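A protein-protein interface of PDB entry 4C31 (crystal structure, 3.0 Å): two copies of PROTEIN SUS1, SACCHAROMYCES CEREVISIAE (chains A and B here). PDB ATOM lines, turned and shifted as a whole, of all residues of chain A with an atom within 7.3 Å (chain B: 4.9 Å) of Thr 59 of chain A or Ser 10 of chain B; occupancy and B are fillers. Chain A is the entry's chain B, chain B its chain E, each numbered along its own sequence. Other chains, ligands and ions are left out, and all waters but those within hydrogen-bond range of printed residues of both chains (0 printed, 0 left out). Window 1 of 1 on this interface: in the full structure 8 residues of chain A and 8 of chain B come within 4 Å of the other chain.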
ATOM      1  N   THR A  56      33.328  16.518   6.397  1.00  0.00           N
ATOM      2  CA  THR A  56      32.607  17.784   6.337  1.00  0.00           C
ATOM      3  C   THR A  56      31.291  17.632   5.590  1.00  0.00           C
ATOM      4  O   THR A  56      31.258  17.624   4.359  1.00  0.00           O
ATOM      5  CB  THR A  56      33.431  18.898   5.685  1.00  0.00           C
ATOM      6  OG1 THR A  56      34.816  18.734   6.016  1.00  0.00           O
ATOM      7  CG2 THR A  56      32.934  20.244   6.198  1.00  0.00           C
ATOM      8  N   ASN A  57      30.208  17.503   6.345  1.00  0.00           N
ATOM      9  CA  ASN A  57      28.885  17.358   5.763  1.00  0.00           C
ATOM     10  C   ASN A  57      28.164  18.701   5.766  1.00  0.00           C
ATOM     11  O   ASN A  57      28.304  19.486   6.701  1.00  0.00           O
ATOM     12  CB  ASN A  57      28.083  16.315   6.537  1.00  0.00           C
ATOM     13  CG  ASN A  57      26.646  16.238   6.084  1.00  0.00           C
ATOM     14  OD1 ASN A  57      25.729  16.214   6.902  1.00  0.00           O
ATOM     15  ND2 ASN A  57      26.437  16.205   4.772  1.00  0.00           N
ATOM     16  N   PHE A  58      27.408  18.969   4.706  1.00  0.00           N
ATOM     17  CA  PHE A  58      26.723  20.251   4.560  1.00  0.00           C
ATOM     18  C   PHE A  58      25.757  20.540   5.702  1.00  0.00           C
ATOM     19  O   PHE A  58      25.774  21.628   6.270  1.00  0.00           O
ATOM     20  CB  PHE A  58      25.962  20.308   3.235  1.00  0.00           C
ATOM     21  CG  PHE A  58      25.086  21.521   3.095  1.00  0.00           C
ATOM     22  CD1 PHE A  58      25.640  22.774   2.887  1.00  0.00           C
ATOM     23  CD2 PHE A  58      23.710  21.412   3.185  1.00  0.00           C
ATOM     24  CE1 PHE A  58      24.835  23.894   2.767  1.00  0.00           C
ATOM     25  CE2 PHE A  58      22.901  22.526   3.064  1.00  0.00           C
ATOM     26  CZ  PHE A  58      23.465  23.767   2.854  1.00  0.00           C
ATOM     27  N   THR A  59      24.907  19.576   6.033  1.00  0.00           N
ATOM     28  CA  THR A  59      23.931  19.785   7.091  1.00  0.00           C
ATOM     29  C   THR A  59      24.650  20.037   8.413  1.00  0.00           C
ATOM     30  O   THR A  59      24.138  20.737   9.289  1.00  0.00           O
ATOM     31  CB  THR A  59      22.989  18.581   7.237  1.00  0.00           C
ATOM     32  OG1 THR A  59      23.754  17.410   7.550  1.00  0.00           O
ATOM     33  CG2 THR A  59      22.216  18.351   5.943  1.00  0.00           C
ATOM     34  N   GLN A  60      25.848  19.476   8.538  1.00  0.00           N
ATOM     35  CA  GLN A  60      26.644  19.636   9.747  1.00  0.00           C
ATOM     36  C   GLN A  60      27.182  21.059   9.878  1.00  0.00           C
ATOM     37  O   GLN A  60      27.007  21.698  10.915  1.00  0.00           O
ATOM     38  CB  GLN A  60      27.800  18.634   9.758  1.00  0.00           C
ATOM     39  CG  GLN A  60      28.652  18.676  11.012  1.00  0.00           C
ATOM     40  CD  GLN A  60      29.805  17.694  10.958  1.00  0.00           C
ATOM     41  OE1 GLN A  60      29.989  16.989   9.966  1.00  0.00           O
ATOM     42  NE2 GLN A  60      30.592  17.650  12.027  1.00  0.00           N
ATOM     43  N   ILE A  61      27.824  21.557   8.825  1.00  0.00           N
ATOM     44  CA  ILE A  61      28.414  22.893   8.861  1.00  0.00           C
ATOM     45  C   ILE A  61      27.327  23.961   8.738  1.00  0.00           C
ATOM     46  O   ILE A  61      27.541  25.119   9.094  1.00  0.00           O
ATOM     47  CB  ILE A  61      29.466  23.090   7.746  1.00  0.00           C
ATOM     48  CG1 ILE A  61      28.806  23.198   6.374  1.00  0.00           C
ATOM     49  CG2 ILE A  61      30.483  21.963   7.764  1.00  0.00           C
ATOM     50  CD1 ILE A  61      28.655  24.619   5.886  1.00  0.00           C
ATOM     51  N   LEU A  62      26.174  23.572   8.205  1.00  0.00           N
ATOM     52  CA  LEU A  62      25.033  24.473   8.109  1.00  0.00           C
ATOM     53  C   LEU A  62      24.681  25.006   9.494  1.00  0.00           C
ATOM     54  O   LEU A  62      24.378  26.183   9.660  1.00  0.00           O
ATOM     55  CB  LEU A  62      23.829  23.752   7.496  1.00  0.00           C
ATOM     56  CG  LEU A  62      22.534  24.548   7.330  1.00  0.00           C
ATOM     57  CD1 LEU A  62      22.654  25.534   6.181  1.00  0.00           C
ATOM     58  CD2 LEU A  62      21.359  23.609   7.114  1.00  0.00           C
ATOM     59  N   SER A  63      24.734  24.124  10.485  1.00  0.00           N
ATOM     60  CA  SER A  63      24.355  24.467  11.851  1.00  0.00           C
ATOM     61  C   SER A  63      25.336  25.423  12.533  1.00  0.00           C
ATOM     62  O   SER A  63      24.975  26.095  13.497  1.00  0.00           O
ATOM     63  CB  SER A  63      24.219  23.193  12.684  1.00  0.00           C
ATOM     64  OG  SER A  63      25.441  22.478  12.714  1.00  0.00           O
ATOM     65  N   THR A  64      26.569  25.480  12.038  1.00  0.00           N
ATOM     66  CA  THR A  64      27.603  26.319  12.645  1.00  0.00           C
ATOM     67  C   THR A  64      27.828  27.617  11.866  1.00  0.00           C
ATOM     68  O   THR A  64      28.393  28.575  12.399  1.00  0.00           O
ATOM     69  CB  THR A  64      28.950  25.567  12.751  1.00  0.00           C
ATOM     70  OG1 THR A  64      29.602  25.542  11.475  1.00  0.00           O
ATOM     71  CG2 THR A  64      28.738  24.142  13.250  1.00  0.00           C
ATOM     72  N   ALA B   6      18.967  10.946   8.184  1.00  0.00           N
ATOM     73  CA  ALA B   6      18.754  12.088   7.306  1.00  0.00           C
ATOM     74  C   ALA B   6      20.080  12.759   6.980  1.00  0.00           C
ATOM     75  O   ALA B   6      20.185  13.509   6.009  1.00  0.00           O
ATOM     76  CB  ALA B   6      17.800  13.079   7.947  1.00  0.00           C
ATOM     77  N   GLN B   7      21.092  12.487   7.797  1.00  0.00           N
ATOM     78  CA  GLN B   7      22.408  13.072   7.598  1.00  0.00           C
ATOM     79  C   GLN B   7      23.244  12.233   6.637  1.00  0.00           C
ATOM     80  O   GLN B   7      24.169  12.739   6.003  1.00  0.00           O
ATOM     81  CB  GLN B   7      23.130  13.218   8.933  1.00  0.00           C
ATOM     82  CG  GLN B   7      24.418  14.008   8.841  1.00  0.00           C
ATOM     83  CD  GLN B   7      24.994  14.325  10.199  1.00  0.00           C
ATOM     84  OE1 GLN B   7      24.499  13.847  11.222  1.00  0.00           O
ATOM     85  NE2 GLN B   7      26.046  15.136  10.223  1.00  0.00           N
ATOM     86  N   LEU B   8      22.921  10.945   6.546  1.00  0.00           N
ATOM     87  CA  LEU B   8      23.569  10.054   5.587  1.00  0.00           C
ATOM     88  C   LEU B   8      23.094  10.351   4.168  1.00  0.00           C
ATOM     89  O   LEU B   8      23.886  10.338   3.227  1.00  0.00           O
ATOM     90  CB  LEU B   8      23.295   8.592   5.937  1.00  0.00           C
ATOM     91  CG  LEU B   8      24.095   8.018   7.109  1.00  0.00           C
ATOM     92  CD1 LEU B   8      23.572   6.638   7.477  1.00  0.00           C
ATOM     93  CD2 LEU B   8      25.583   7.953   6.786  1.00  0.00           C
ATOM     94  N   LYS B   9      21.799  10.615   4.022  1.00  0.00           N
ATOM     95  CA  LYS B   9      21.235  11.001   2.733  1.00  0.00           C
ATOM     96  C   LYS B   9      21.895  12.286   2.237  1.00  0.00           C
ATOM     97  O   LYS B   9      21.977  12.532   1.035  1.00  0.00           O
ATOM     98  CB  LYS B   9      19.719  11.197   2.833  1.00  0.00           C
ATOM     99  CG  LYS B   9      18.980  10.023   3.447  1.00  0.00           C
ATOM    100  CD  LYS B   9      17.696   9.692   2.702  1.00  0.00           C
ATOM    101  CE  LYS B   9      16.698  10.829   2.744  1.00  0.00           C
ATOM    102  NZ  LYS B   9      15.413  10.436   2.102  1.00  0.00           N
ATOM    103  N   SER B  10      22.365  13.108   3.170  1.00  0.00           N
ATOM    104  CA  SER B  10      23.064  14.328   2.804  1.00  0.00           C
ATOM    105  C   SER B  10      24.428  13.981   2.222  1.00  0.00           C
ATOM    106  O   SER B  10      24.848  14.562   1.223  1.00  0.00           O
ATOM    107  CB  SER B  10      23.220  15.251   4.015  1.00  0.00           C
ATOM    108  OG  SER B  10      23.721  16.520   3.624  1.00  0.00           O
ATOM    109  N   GLN B  11      25.113  13.029   2.845  1.00  0.00           N
ATOM    110  CA  GLN B  11      26.425  12.591   2.371  1.00  0.00           C
ATOM    111  C   GLN B  11      26.343  11.872   1.024  1.00  0.00           C
ATOM    112  O   GLN B  11      27.202  12.061   0.162  1.00  0.00           O
ATOM    113  CB  GLN B  11      27.095  11.687   3.406  1.00  0.00           C
ATOM    114  CG  GLN B  11      27.619  12.435   4.618  1.00  0.00           C
ATOM    115  CD  GLN B  11      28.958  11.907   5.089  1.00  0.00           C
ATOM    116  OE1 GLN B  11      29.993  12.543   4.886  1.00  0.00           O
ATOM    117  NE2 GLN B  11      28.945  10.738   5.721  1.00  0.00           N
ATOM    118  N   ILE B  12      25.321  11.036   0.855  1.00  0.00           N
ATOM    119  CA  ILE B  12      25.075  10.369  -0.423  1.00  0.00           C
ATOM    120  C   ILE B  12      24.891  11.395  -1.537  1.00  0.00           C
ATOM    121  O   ILE B  12      25.609  11.375  -2.540  1.00  0.00           O
ATOM    122  CB  ILE B  12      23.829   9.459  -0.354  1.00  0.00           C
ATOM    123  CG1 ILE B  12      24.085   8.285   0.589  1.00  0.00           C
ATOM    124  CG2 ILE B  12      23.460   8.931  -1.741  1.00  0.00           C
ATOM    125  CD1 ILE B  12      22.857   7.434   0.877  1.00  0.00           C
ATOM    126  N   GLN B  13      23.919  12.286  -1.356  1.00  0.00           N
ATOM    127  CA  GLN B  13      23.617  13.305  -2.354  1.00  0.00           C
ATOM    128  C   GLN B  13      24.830  14.178  -2.625  1.00  0.00           C
ATOM    129  O   GLN B  13      25.056  14.604  -3.757  1.00  0.00           O
ATOM    130  CB  GLN B  13      22.446  14.177  -1.905  1.00  0.00           C
ATOM    131  CG  GLN B  13      21.889  15.053  -3.015  1.00  0.00           C
ATOM    132  CD  GLN B  13      20.832  16.017  -2.525  1.00  0.00           C
ATOM    133  OE1 GLN B  13      19.638  15.708  -2.528  1.00  0.00           O
ATOM    134  NE2 GLN B  13      21.267  17.196  -2.096  1.00  0.00           N
ATOM    135  N   GLN B  14      25.605  14.448  -1.581  1.00  0.00           N
ATOM    136  CA  GLN B  14      26.800  15.267  -1.719  1.00  0.00           C
ATOM    137  C   GLN B  14      27.737  14.608  -2.715  1.00  0.00           C
ATOM    138  O   GLN B  14      28.120  15.205  -3.724  1.00  0.00           O
ATOM    139  CB  GLN B  14      27.489  15.457  -0.364  1.00  0.00           C
ATOM    140  CG  GLN B  14      28.766  16.292  -0.409  1.00  0.00           C
ATOM    141  CD  GLN B  14      29.608  16.181   0.858  1.00  0.00           C
ATOM    142  OE1 GLN B  14      30.788  16.523   0.851  1.00  0.00           O
ATOM    143  NE2 GLN B  14      29.003  15.716   1.951  1.00  0.00           N
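No position is printed for both chains. Of the 8 pairs that touch across the chains among the printed residues, none has its exchanged pair printed and touching as well.
Among the printed residues, pairs that only touch across the chains: Thr 56 of chain A with Gln 14 of chain B (3.7 Å), Asn 57 of chain A with Gln 7 of chain B (3.2 Å), Asn 57 of chain A with Gln 11 of chain B (3.9 Å), Asn 57 of chain A with Gln 14 of chain B (3.8 Å), Thr 59 of chain A with Gln 7 of chain B (3.7 Å), Thr 59 of chain A with Ser 10 of chain B (3.3 Å) and Gln 60 of chain A with Gln 7 of chain B (3.9 Å).
Of the printed residues of chain B, Thr 56 of chain A touches Gln 14. Thr 59 of chain A touches just these residues of chain B: Gln 7 and Ser 10. Of the printed residues of chain A, Gln 7 of chain B touches Asn 57, Thr 59 and Gln 60. Ser 10 of chain B touches just these residues of chain A: Asn 57 (3.0 Å) and Thr 59 (3.3 Å).
ND2 of Asn 57 of chain A lies within hydrogen-bond range of OG of Ser 10 of chain B, 3.0 Å away.
The side-chain hydroxyl (OG) of Ser 63 of chain A sits at hydrogen-bond distance from the backbone carbonyl oxygen (O) of Gln 60 of chain A (2.5 Å).
Of the 9 printed residues of chain A, 4 touch a printed residue of chain B.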
